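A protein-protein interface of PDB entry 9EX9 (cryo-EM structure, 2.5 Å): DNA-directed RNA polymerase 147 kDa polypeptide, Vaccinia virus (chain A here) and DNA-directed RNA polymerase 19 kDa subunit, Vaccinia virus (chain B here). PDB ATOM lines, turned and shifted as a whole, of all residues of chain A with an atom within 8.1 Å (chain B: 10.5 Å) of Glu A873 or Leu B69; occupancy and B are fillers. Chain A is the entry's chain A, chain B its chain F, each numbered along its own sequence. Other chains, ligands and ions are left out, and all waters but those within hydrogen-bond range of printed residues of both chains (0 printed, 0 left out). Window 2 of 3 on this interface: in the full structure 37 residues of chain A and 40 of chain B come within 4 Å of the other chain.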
ATOM      1  N   TYR A 771      10.135 -31.566  25.857  1.00  0.00           N
ATOM      2  CA  TYR A 771      10.717 -30.232  25.830  1.00  0.00           C
ATOM      3  C   TYR A 771       9.906 -29.227  26.634  1.00  0.00           C
ATOM      4  O   TYR A 771      10.044 -28.021  26.423  1.00  0.00           O
ATOM      5  CB  TYR A 771      10.854 -29.742  24.394  1.00  0.00           C
ATOM      6  CG  TYR A 771      11.691 -30.626  23.511  1.00  0.00           C
ATOM      7  CD1 TYR A 771      13.070 -30.606  23.583  1.00  0.00           C
ATOM      8  CD2 TYR A 771      11.100 -31.469  22.590  1.00  0.00           C
ATOM      9  CE1 TYR A 771      13.832 -31.409  22.772  1.00  0.00           C
ATOM     10  CE2 TYR A 771      11.856 -32.272  21.775  1.00  0.00           C
ATOM     11  CZ  TYR A 771      13.219 -32.235  21.867  1.00  0.00           C
ATOM     12  OH  TYR A 771      13.972 -33.037  21.052  1.00  0.00           O
ATOM     13  N   ASN A 866      21.458 -10.825  33.229  1.00  0.00           N
ATOM     14  CA  ASN A 866      22.170 -11.912  32.575  1.00  0.00           C
ATOM     15  C   ASN A 866      21.487 -13.248  32.819  1.00  0.00           C
ATOM     16  O   ASN A 866      21.384 -14.073  31.904  1.00  0.00           O
ATOM     17  CB  ASN A 866      23.616 -11.949  33.059  1.00  0.00           C
ATOM     18  CG  ASN A 866      24.404 -10.739  32.619  1.00  0.00           C
ATOM     19  OD1 ASN A 866      24.080 -10.108  31.617  1.00  0.00           O
ATOM     20  ND2 ASN A 866      25.451 -10.412  33.361  1.00  0.00           N
ATOM     21  N   VAL A 867      21.011 -13.488  34.042  1.00  0.00           N
ATOM     22  CA  VAL A 867      20.310 -14.735  34.315  1.00  0.00           C
ATOM     23  C   VAL A 867      19.065 -14.840  33.450  1.00  0.00           C
ATOM     24  O   VAL A 867      18.768 -15.904  32.891  1.00  0.00           O
ATOM     25  CB  VAL A 867      19.966 -14.841  35.810  1.00  0.00           C
ATOM     26  CG1 VAL A 867      18.941 -15.930  36.037  1.00  0.00           C
ATOM     27  CG2 VAL A 867      21.213 -15.122  36.610  1.00  0.00           C
ATOM     28  N   ILE A 868      18.311 -13.749  33.330  1.00  0.00           N
ATOM     29  CA  ILE A 868      17.083 -13.810  32.546  1.00  0.00           C
ATOM     30  C   ILE A 868      17.397 -14.067  31.078  1.00  0.00           C
ATOM     31  O   ILE A 868      16.727 -14.872  30.429  1.00  0.00           O
ATOM     32  CB  ILE A 868      16.253 -12.532  32.737  1.00  0.00           C
ATOM     33  CG1 ILE A 868      15.660 -12.491  34.149  1.00  0.00           C
ATOM     34  CG2 ILE A 868      15.155 -12.460  31.703  1.00  0.00           C
ATOM     35  CD1 ILE A 868      14.706 -13.621  34.462  1.00  0.00           C
ATOM     36  N   ASP A 869      18.415 -13.402  30.531  1.00  0.00           N
ATOM     37  CA  ASP A 869      18.768 -13.656  29.134  1.00  0.00           C
ATOM     38  C   ASP A 869      19.200 -15.104  28.921  1.00  0.00           C
ATOM     39  O   ASP A 869      18.799 -15.753  27.940  1.00  0.00           O
ATOM     40  CB  ASP A 869      19.876 -12.706  28.692  1.00  0.00           C
ATOM     41  CG  ASP A 869      19.372 -11.309  28.417  1.00  0.00           C
ATOM     42  OD1 ASP A 869      18.142 -11.115  28.360  1.00  0.00           O
ATOM     43  OD2 ASP A 869      20.208 -10.399  28.254  1.00  0.00           O
ATOM     44  N   ASP A 870      20.020 -15.628  29.834  1.00  0.00           N
ATOM     45  CA  ASP A 870      20.483 -17.005  29.717  1.00  0.00           C
ATOM     46  C   ASP A 870      19.312 -17.974  29.712  1.00  0.00           C
ATOM     47  O   ASP A 870      19.201 -18.828  28.827  1.00  0.00           O
ATOM     48  CB  ASP A 870      21.438 -17.316  30.866  1.00  0.00           C
ATOM     49  CG  ASP A 870      21.910 -18.746  30.861  1.00  0.00           C
ATOM     50  OD1 ASP A 870      22.720 -19.102  29.983  1.00  0.00           O
ATOM     51  OD2 ASP A 870      21.482 -19.516  31.743  1.00  0.00           O
ATOM     52  N   VAL A 871      18.417 -17.844  30.692  1.00  0.00           N
ATOM     53  CA  VAL A 871      17.271 -18.743  30.771  1.00  0.00           C
ATOM     54  C   VAL A 871      16.354 -18.556  29.577  1.00  0.00           C
ATOM     55  O   VAL A 871      15.707 -19.507  29.126  1.00  0.00           O
ATOM     56  CB  VAL A 871      16.520 -18.521  32.091  1.00  0.00           C
ATOM     57  CG1 VAL A 871      15.153 -19.159  32.035  1.00  0.00           C
ATOM     58  CG2 VAL A 871      17.319 -19.084  33.239  1.00  0.00           C
ATOM     59  N   ARG A 872      16.261 -17.336  29.057  1.00  0.00           N
ATOM     60  CA  ARG A 872      15.395 -17.082  27.917  1.00  0.00           C
ATOM     61  C   ARG A 872      15.870 -17.838  26.691  1.00  0.00           C
ATOM     62  O   ARG A 872      15.057 -18.383  25.939  1.00  0.00           O
ATOM     63  CB  ARG A 872      15.348 -15.583  27.645  1.00  0.00           C
ATOM     64  CG  ARG A 872      14.465 -15.164  26.499  1.00  0.00           C
ATOM     65  CD  ARG A 872      14.572 -13.670  26.293  1.00  0.00           C
ATOM     66  NE  ARG A 872      14.244 -12.935  27.507  1.00  0.00           N
ATOM     67  CZ  ARG A 872      14.620 -11.689  27.755  1.00  0.00           C
ATOM     68  NH1 ARG A 872      15.365 -11.008  26.902  1.00  0.00           N
ATOM     69  NH2 ARG A 872      14.241 -11.112  28.891  1.00  0.00           N
ATOM     70  N   GLU A 873      17.182 -17.880  26.459  1.00  0.00           N
ATOM     71  CA  GLU A 873      17.641 -18.593  25.269  1.00  0.00           C
ATOM     72  C   GLU A 873      17.791 -20.096  25.496  1.00  0.00           C
ATOM     73  O   GLU A 873      17.570 -20.873  24.564  1.00  0.00           O
ATOM     74  CB  GLU A 873      18.958 -18.015  24.760  1.00  0.00           C
ATOM     75  CG  GLU A 873      20.136 -18.195  25.681  1.00  0.00           C
ATOM     76  CD  GLU A 873      21.453 -18.023  24.959  1.00  0.00           C
ATOM     77  OE1 GLU A 873      21.562 -18.492  23.805  1.00  0.00           O
ATOM     78  OE2 GLU A 873      22.376 -17.415  25.543  1.00  0.00           O
ATOM     79  N   LYS A 874      18.150 -20.535  26.703  1.00  0.00           N
ATOM     80  CA  LYS A 874      18.508 -21.937  26.899  1.00  0.00           C
ATOM     81  C   LYS A 874      17.333 -22.835  27.247  1.00  0.00           C
ATOM     82  O   LYS A 874      17.351 -24.014  26.885  1.00  0.00           O
ATOM     83  CB  LYS A 874      19.562 -22.068  27.998  1.00  0.00           C
ATOM     84  CG  LYS A 874      20.960 -21.748  27.530  1.00  0.00           C
ATOM     85  CD  LYS A 874      21.975 -21.973  28.623  1.00  0.00           C
ATOM     86  CE  LYS A 874      23.337 -21.456  28.217  1.00  0.00           C
ATOM     87  NZ  LYS A 874      24.339 -21.639  29.299  1.00  0.00           N
ATOM     88  N   TYR A 875      16.317 -22.327  27.941  1.00  0.00           N
ATOM     89  CA  TYR A 875      15.199 -23.156  28.370  1.00  0.00           C
ATOM     90  C   TYR A 875      13.894 -22.859  27.651  1.00  0.00           C
ATOM     91  O   TYR A 875      12.988 -23.693  27.694  1.00  0.00           O
ATOM     92  CB  TYR A 875      14.974 -23.000  29.878  1.00  0.00           C
ATOM     93  CG  TYR A 875      16.029 -23.680  30.713  1.00  0.00           C
ATOM     94  CD1 TYR A 875      17.231 -23.055  30.991  1.00  0.00           C
ATOM     95  CD2 TYR A 875      15.820 -24.949  31.223  1.00  0.00           C
ATOM     96  CE1 TYR A 875      18.194 -23.675  31.750  1.00  0.00           C
ATOM     97  CE2 TYR A 875      16.774 -25.574  31.981  1.00  0.00           C
ATOM     98  CZ  TYR A 875      17.960 -24.934  32.242  1.00  0.00           C
ATOM     99  OH  TYR A 875      18.914 -25.560  33.000  1.00  0.00           O
ATOM    100  N   PHE A 876      13.770 -21.702  27.010  1.00  0.00           N
ATOM    101  CA  PHE A 876      12.586 -21.366  26.237  1.00  0.00           C
ATOM    102  C   PHE A 876      12.886 -21.204  24.756  1.00  0.00           C
ATOM    103  O   PHE A 876      11.974 -20.915  23.978  1.00  0.00           O
ATOM    104  CB  PHE A 876      11.942 -20.092  26.794  1.00  0.00           C
ATOM    105  CG  PHE A 876      11.385 -20.262  28.178  1.00  0.00           C
ATOM    106  CD1 PHE A 876      12.183 -20.072  29.286  1.00  0.00           C
ATOM    107  CD2 PHE A 876      10.068 -20.626  28.370  1.00  0.00           C
ATOM    108  CE1 PHE A 876      11.678 -20.236  30.551  1.00  0.00           C
ATOM    109  CE2 PHE A 876       9.563 -20.790  29.635  1.00  0.00           C
ATOM    110  CZ  PHE A 876      10.370 -20.593  30.724  1.00  0.00           C
ATOM    111  N   PHE A 877      14.139 -21.385  24.347  1.00  0.00           N
ATOM    112  CA  PHE A 877      14.501 -21.510  22.939  1.00  0.00           C
ATOM    113  C   PHE A 877      14.157 -20.256  22.143  1.00  0.00           C
ATOM    114  O   PHE A 877      13.919 -20.325  20.937  1.00  0.00           O
ATOM    115  CB  PHE A 877      13.835 -22.737  22.314  1.00  0.00           C
ATOM    116  CG  PHE A 877      13.992 -23.991  23.127  1.00  0.00           C
ATOM    117  CD1 PHE A 877      15.180 -24.279  23.761  1.00  0.00           C
ATOM    118  CD2 PHE A 877      12.945 -24.877  23.264  1.00  0.00           C
ATOM    119  CE1 PHE A 877      15.318 -25.421  24.509  1.00  0.00           C
ATOM    120  CE2 PHE A 877      13.085 -26.019  24.015  1.00  0.00           C
ATOM    121  CZ  PHE A 877      14.271 -26.288  24.634  1.00  0.00           C
ATOM    122  N   THR A 878      14.141 -19.099  22.795  1.00  0.00           N
ATOM    123  CA  THR A 878      14.006 -17.804  22.133  1.00  0.00           C
ATOM    124  C   THR A 878      12.619 -17.564  21.560  1.00  0.00           C
ATOM    125  O   THR A 878      12.453 -16.698  20.700  1.00  0.00           O
ATOM    126  CB  THR A 878      15.029 -17.644  21.004  1.00  0.00           C
ATOM    127  OG1 THR A 878      14.687 -18.520  19.926  1.00  0.00           O
ATOM    128  CG2 THR A 878      16.423 -17.966  21.486  1.00  0.00           C
ATOM    129  N   VAL A 879      11.612 -18.302  22.005  1.00  0.00           N
ATOM    130  CA  VAL A 879      10.263 -18.171  21.473  1.00  0.00           C
ATOM    131  C   VAL A 879       9.337 -17.484  22.463  1.00  0.00           C
ATOM    132  O   VAL A 879       8.718 -16.470  22.143  1.00  0.00           O
ATOM    133  CB  VAL A 879       9.718 -19.556  21.064  1.00  0.00           C
ATOM    134  CG1 VAL A 879       8.219 -19.505  20.890  1.00  0.00           C
ATOM    135  CG2 VAL A 879      10.379 -20.018  19.787  1.00  0.00           C
ATOM    136  N   SER A 880       9.238 -18.012  23.677  1.00  0.00           N
ATOM    137  CA  SER A 880       8.304 -17.486  24.656  1.00  0.00           C
ATOM    138  C   SER A 880       8.774 -16.134  25.183  1.00  0.00           C
ATOM    139  O   SER A 880       9.891 -15.683  24.927  1.00  0.00           O
ATOM    140  CB  SER A 880       8.132 -18.469  25.809  1.00  0.00           C
ATOM    141  OG  SER A 880       7.602 -19.696  25.349  1.00  0.00           O
ATOM    142  N   ILE A 882       9.122 -14.030  28.737  1.00  0.00           N
ATOM    143  CA  ILE A 882       9.179 -14.214  30.184  1.00  0.00           C
ATOM    144  C   ILE A 882       9.527 -12.902  30.872  1.00  0.00           C
ATOM    145  O   ILE A 882      10.214 -12.893  31.897  1.00  0.00           O
ATOM    146  CB  ILE A 882      10.178 -15.317  30.566  1.00  0.00           C
ATOM    147  CG1 ILE A 882      11.568 -15.003  30.017  1.00  0.00           C
ATOM    148  CG2 ILE A 882       9.697 -16.646  30.043  1.00  0.00           C
ATOM    149  CD1 ILE A 882      12.630 -15.957  30.489  1.00  0.00           C
ATOM    150  N   ILE B  62      20.901 -21.615  11.777  1.00  0.00           N
ATOM    151  CA  ILE B  62      20.219 -21.242  13.010  1.00  0.00           C
ATOM    152  C   ILE B  62      19.436 -22.435  13.533  1.00  0.00           C
ATOM    153  O   ILE B  62      19.117 -22.505  14.716  1.00  0.00           O
ATOM    154  CB  ILE B  62      19.298 -20.027  12.792  1.00  0.00           C
ATOM    155  CG1 ILE B  62      18.748 -19.520  14.127  1.00  0.00           C
ATOM    156  CG2 ILE B  62      18.155 -20.384  11.861  1.00  0.00           C
ATOM    157  CD1 ILE B  62      19.810 -19.005  15.082  1.00  0.00           C
ATOM    158  N   GLY B  63      19.114 -23.371  12.639  1.00  0.00           N
ATOM    159  CA  GLY B  63      18.530 -24.625  13.075  1.00  0.00           C
ATOM    160  C   GLY B  63      19.490 -25.469  13.884  1.00  0.00           C
ATOM    161  O   GLY B  63      19.074 -26.196  14.790  1.00  0.00           O
ATOM    162  N   ASN B  64      20.784 -25.393  13.569  1.00  0.00           N
ATOM    163  CA  ASN B  64      21.776 -26.134  14.337  1.00  0.00           C
ATOM    164  C   ASN B  64      21.839 -25.637  15.773  1.00  0.00           C
ATOM    165  O   ASN B  64      21.989 -26.431  16.707  1.00  0.00           O
ATOM    166  CB  ASN B  64      23.142 -26.017  13.668  1.00  0.00           C
ATOM    167  CG  ASN B  64      23.136 -26.530  12.246  1.00  0.00           C
ATOM    168  OD1 ASN B  64      23.444 -25.796  11.308  1.00  0.00           O
ATOM    169  ND2 ASN B  64      22.780 -27.797  12.077  1.00  0.00           N
ATOM    170  N   HIS B  65      21.732 -24.324  15.968  1.00  0.00           N
ATOM    171  CA  HIS B  65      21.770 -23.771  17.315  1.00  0.00           C
ATOM    172  C   HIS B  65      20.609 -24.293  18.152  1.00  0.00           C
ATOM    173  O   HIS B  65      20.791 -24.723  19.299  1.00  0.00           O
ATOM    174  CB  HIS B  65      21.741 -22.247  17.236  1.00  0.00           C
ATOM    175  CG  HIS B  65      22.137 -21.567  18.507  1.00  0.00           C
ATOM    176  ND1 HIS B  65      23.235 -21.951  19.244  1.00  0.00           N
ATOM    177  CD2 HIS B  65      21.589 -20.519  19.164  1.00  0.00           C
ATOM    178  CE1 HIS B  65      23.343 -21.173  20.306  1.00  0.00           C
ATOM    179  NE2 HIS B  65      22.357 -20.295  20.280  1.00  0.00           N
ATOM    180  N   ILE B  66      19.404 -24.275  17.585  1.00  0.00           N
ATOM    181  CA  ILE B  66      18.237 -24.755  18.315  1.00  0.00           C
ATOM    182  C   ILE B  66      18.341 -26.253  18.555  1.00  0.00           C
ATOM    183  O   ILE B  66      17.948 -26.756  19.613  1.00  0.00           O
ATOM    184  CB  ILE B  66      16.949 -24.389  17.558  1.00  0.00           C
ATOM    185  CG1 ILE B  66      16.857 -22.877  17.339  1.00  0.00           C
ATOM    186  CG2 ILE B  66      15.734 -24.888  18.313  1.00  0.00           C
ATOM    187  CD1 ILE B  66      16.774 -22.066  18.612  1.00  0.00           C
ATOM    188  N   SER B  67      18.872 -26.993  17.581  1.00  0.00           N
ATOM    189  CA  SER B  67      19.055 -28.426  17.769  1.00  0.00           C
ATOM    190  C   SER B  67      19.999 -28.709  18.927  1.00  0.00           C
ATOM    191  O   SER B  67      19.742 -29.601  19.743  1.00  0.00           O
ATOM    192  CB  SER B  67      19.584 -29.054  16.485  1.00  0.00           C
ATOM    193  OG  SER B  67      18.751 -28.733  15.388  1.00  0.00           O
ATOM    194  N   ALA B  68      21.101 -27.961  19.013  1.00  0.00           N
ATOM    195  CA  ALA B  68      22.041 -28.148  20.112  1.00  0.00           C
ATOM    196  C   ALA B  68      21.403 -27.802  21.449  1.00  0.00           C
ATOM    197  O   ALA B  68      21.583 -28.524  22.440  1.00  0.00           O
ATOM    198  CB  ALA B  68      23.285 -27.297  19.879  1.00  0.00           C
ATOM    199  N   LEU B  69      20.655 -26.700  21.501  1.00  0.00           N
ATOM    200  CA  LEU B  69      19.990 -26.341  22.748  1.00  0.00           C
ATOM    201  C   LEU B  69      19.025 -27.433  23.182  1.00  0.00           C
ATOM    202  O   LEU B  69      18.964 -27.784  24.364  1.00  0.00           O
ATOM    203  CB  LEU B  69      19.252 -25.011  22.594  1.00  0.00           C
ATOM    204  CG  LEU B  69      20.102 -23.746  22.501  1.00  0.00           C
ATOM    205  CD1 LEU B  69      19.221 -22.553  22.215  1.00  0.00           C
ATOM    206  CD2 LEU B  69      20.886 -23.524  23.776  1.00  0.00           C
ATOM    207  N   LYS B  70      18.268 -27.990  22.240  1.00  0.00           N
ATOM    208  CA  LYS B  70      17.316 -29.040  22.582  1.00  0.00           C
ATOM    209  C   LYS B  70      18.025 -30.322  23.015  1.00  0.00           C
ATOM    210  O   LYS B  70      17.571 -31.012  23.937  1.00  0.00           O
ATOM    211  CB  LYS B  70      16.393 -29.290  21.393  1.00  0.00           C
ATOM    212  CG  LYS B  70      15.506 -28.096  21.059  1.00  0.00           C
ATOM    213  CD  LYS B  70      14.743 -28.281  19.759  1.00  0.00           C
ATOM    214  CE  LYS B  70      13.643 -29.312  19.891  1.00  0.00           C
ATOM    215  NZ  LYS B  70      12.972 -29.579  18.595  1.00  0.00           N
ATOM    216  N   ARG B  71      19.142 -30.658  22.367  1.00  0.00           N
ATOM    217  CA  ARG B  71      19.908 -31.826  22.789  1.00  0.00           C
ATOM    218  C   ARG B  71      20.398 -31.669  24.219  1.00  0.00           C
ATOM    219  O   ARG B  71      20.339 -32.616  25.009  1.00  0.00           O
ATOM    220  CB  ARG B  71      21.089 -32.058  21.853  1.00  0.00           C
ATOM    221  CG  ARG B  71      20.763 -32.899  20.648  1.00  0.00           C
ATOM    222  CD  ARG B  71      22.022 -33.451  20.017  1.00  0.00           C
ATOM    223  NE  ARG B  71      22.926 -32.398  19.574  1.00  0.00           N
ATOM    224  CZ  ARG B  71      22.886 -31.826  18.379  1.00  0.00           C
ATOM    225  NH1 ARG B  71      21.980 -32.167  17.477  1.00  0.00           N
ATOM    226  NH2 ARG B  71      23.778 -30.887  18.080  1.00  0.00           N
ATOM    227  N   ARG B  72      20.897 -30.483  24.570  1.00  0.00           N
ATOM    228  CA  ARG B  72      21.275 -30.246  25.959  1.00  0.00           C
ATOM    229  C   ARG B  72      20.064 -30.342  26.876  1.00  0.00           C
ATOM    230  O   ARG B  72      20.144 -30.921  27.964  1.00  0.00           O
ATOM    231  CB  ARG B  72      21.948 -28.886  26.102  1.00  0.00           C
ATOM    232  CG  ARG B  72      23.362 -28.851  25.570  1.00  0.00           C
ATOM    233  CD  ARG B  72      24.045 -27.533  25.880  1.00  0.00           C
ATOM    234  NE  ARG B  72      24.228 -27.330  27.313  1.00  0.00           N
ATOM    235  CZ  ARG B  72      25.253 -27.796  28.014  1.00  0.00           C
ATOM    236  NH1 ARG B  72      26.212 -28.511  27.449  1.00  0.00           N
ATOM    237  NH2 ARG B  72      25.316 -27.541  29.317  1.00  0.00           N
ATOM    238  N   TYR B  73      18.931 -29.784  26.450  1.00  0.00           N
ATOM    239  CA  TYR B  73      17.717 -29.860  27.253  1.00  0.00           C
ATOM    240  C   TYR B  73      17.327 -31.304  27.531  1.00  0.00           C
ATOM    241  O   TYR B  73      16.719 -31.595  28.563  1.00  0.00           O
ATOM    242  CB  TYR B  73      16.579 -29.130  26.538  1.00  0.00           C
ATOM    243  CG  TYR B  73      15.401 -28.814  27.422  1.00  0.00           C
ATOM    244  CD1 TYR B  73      15.358 -27.646  28.157  1.00  0.00           C
ATOM    245  CD2 TYR B  73      14.336 -29.685  27.524  1.00  0.00           C
ATOM    246  CE1 TYR B  73      14.290 -27.355  28.969  1.00  0.00           C
ATOM    247  CE2 TYR B  73      13.264 -29.402  28.334  1.00  0.00           C
ATOM    248  CZ  TYR B  73      13.246 -28.237  29.054  1.00  0.00           C
ATOM    249  OH  TYR B  73      12.177 -27.952  29.864  1.00  0.00           O
ATOM    250  N   THR B  74      17.672 -32.218  26.627  1.00  0.00           N
ATOM    251  CA  THR B  74      17.279 -33.615  26.789  1.00  0.00           C
ATOM    252  C   THR B  74      17.850 -34.256  28.052  1.00  0.00           C
ATOM    253  O   THR B  74      17.334 -35.288  28.491  1.00  0.00           O
ATOM    254  CB  THR B  74      17.727 -34.423  25.569  1.00  0.00           C
ATOM    255  OG1 THR B  74      17.006 -33.984  24.416  1.00  0.00           O
ATOM    256  CG2 THR B  74      17.489 -35.908  25.777  1.00  0.00           C
ATOM    257  N   ARG B  75      18.893 -33.685  28.647  1.00  0.00           N
ATOM    258  CA  ARG B  75      19.648 -34.367  29.689  1.00  0.00           C
ATOM    259  C   ARG B  75      19.099 -34.152  31.092  1.00  0.00           C
ATOM    260  O   ARG B  75      19.687 -34.668  32.046  1.00  0.00           O
ATOM    261  CB  ARG B  75      21.108 -33.920  29.658  1.00  0.00           C
ATOM    262  CG  ARG B  75      21.805 -34.174  28.346  1.00  0.00           C
ATOM    263  CD  ARG B  75      21.842 -35.644  27.987  1.00  0.00           C
ATOM    264  NE  ARG B  75      22.563 -35.861  26.739  1.00  0.00           N
ATOM    265  CZ  ARG B  75      23.855 -36.144  26.648  1.00  0.00           C
ATOM    266  NH1 ARG B  75      24.608 -36.310  27.721  1.00  0.00           N
ATOM    267  NH2 ARG B  75      24.409 -36.265  25.446  1.00  0.00           N
ATOM    268  N   ARG B  76      18.011 -33.412  31.258  1.00  0.00           N
ATOM    269  CA  ARG B  76      17.457 -33.209  32.589  1.00  0.00           C
ATOM    270  C   ARG B  76      16.581 -34.390  32.983  1.00  0.00           C
ATOM    271  O   ARG B  76      15.984 -35.056  32.137  1.00  0.00           O
ATOM    272  CB  ARG B  76      16.674 -31.896  32.669  1.00  0.00           C
ATOM    273  CG  ARG B  76      15.711 -31.628  31.532  1.00  0.00           C
ATOM    274  CD  ARG B  76      15.346 -30.162  31.451  1.00  0.00           C
ATOM    275  NE  ARG B  76      14.457 -29.776  32.536  1.00  0.00           N
ATOM    276  CZ  ARG B  76      13.178 -30.113  32.603  1.00  0.00           C
ATOM    277  NH1 ARG B  76      12.610 -30.855  31.670  1.00  0.00           N
ATOM    278  NH2 ARG B  76      12.451 -29.698  33.634  1.00  0.00           N
ATOM    279  N   ASN B 133      14.232 -38.667  23.469  1.00  0.00           N
ATOM    280  CA  ASN B 133      13.913 -37.731  22.392  1.00  0.00           C
ATOM    281  C   ASN B 133      14.580 -38.183  21.103  1.00  0.00           C
ATOM    282  O   ASN B 133      15.248 -37.411  20.415  1.00  0.00           O
ATOM    283  CB  ASN B 133      14.339 -36.309  22.749  1.00  0.00           C
ATOM    284  CG  ASN B 133      13.410 -35.650  23.744  1.00  0.00           C
ATOM    285  OD1 ASN B 133      12.228 -35.962  23.804  1.00  0.00           O
ATOM    286  ND2 ASN B 133      13.943 -34.723  24.525  1.00  0.00           N
ATOM    287  N   GLU B 135      16.908 -40.463  21.206  1.00  0.00           N
ATOM    288  CA  GLU B 135      18.223 -40.899  21.640  1.00  0.00           C
ATOM    289  C   GLU B 135      18.068 -42.022  22.653  1.00  0.00           C
ATOM    290  O   GLU B 135      16.971 -42.314  23.127  1.00  0.00           O
ATOM    291  CB  GLU B 135      19.013 -39.738  22.249  1.00  0.00           C
ATOM    292  CG  GLU B 135      19.141 -38.550  21.324  1.00  0.00           C
ATOM    293  CD  GLU B 135      20.022 -37.462  21.890  1.00  0.00           C
ATOM    294  OE1 GLU B 135      20.900 -37.773  22.716  1.00  0.00           O
ATOM    295  OE2 GLU B 135      19.833 -36.292  21.506  1.00  0.00           O
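The backbone carbonyl oxygen (O) of Lys B70 sits at hydrogen-bond distance from the side-chain hydroxyl (OG1) of Thr B74 (3.1 Å).
The guanidinium group (NH1) of Arg B76 is in hydrogen-bond range of the side-chain hydroxyl (OH) of Tyr B73 (3.4 Å).
The side-chain amide nitrogen (ND2) of Asn B133 is in hydrogen-bond range of the side-chain hydroxyl (OG1) of Thr B74 (3.2 Å).
Of the 17 printed residues of chain B, 4 touch a printed residue of chain A.
Hydrophobic or aromatic side chains of chain A within 4 Å of the printed part of chain B: Tyr A771, Tyr A875 and Phe A877.
Among the printed residues, 6 pairs touch across the chains.
Among the printed residues, no Asp or Glu carboxylate lies within 4 Å of a Lys or Arg side-chain nitrogen of the other chain.
Among the printed residues, merely in contact across the chains: Glu A873 with Leu B69 (3.3 Å), Tyr A771 with Lys B70 (3.6 Å), Tyr A875 with Tyr B73 (3.6 Å), Tyr A771 with Tyr B73 (3.7 Å), Tyr A771 with Asn B133 (3.7 Å) and Phe A877 with Tyr B73 (3.9 Å).
Glu A873 touches just one residue of chain B: Leu B69 (3.3 Å).
Of the printed residues of chain A, Leu B69 touches Glu A873 (3.3 Å).
Of the printed residues of chain B, Phe A877 touches Tyr B73 (3.9 Å).
Of the printed residues of chain A, Lys B70 touches Tyr A771.
Of the printed residues of chain A, Tyr B73 touches Tyr A771 (3.7 Å), Tyr A875 (3.6 Å) and Phe A877 (3.9 Å).
Printed residues of chain B within 4 Å of Tyr A875: Tyr B73.
Arg B76 touches none of the printed residues of chain A.
The nearest residue of chain B that does not touch Glu A873 is His B65 (4.04 Å).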
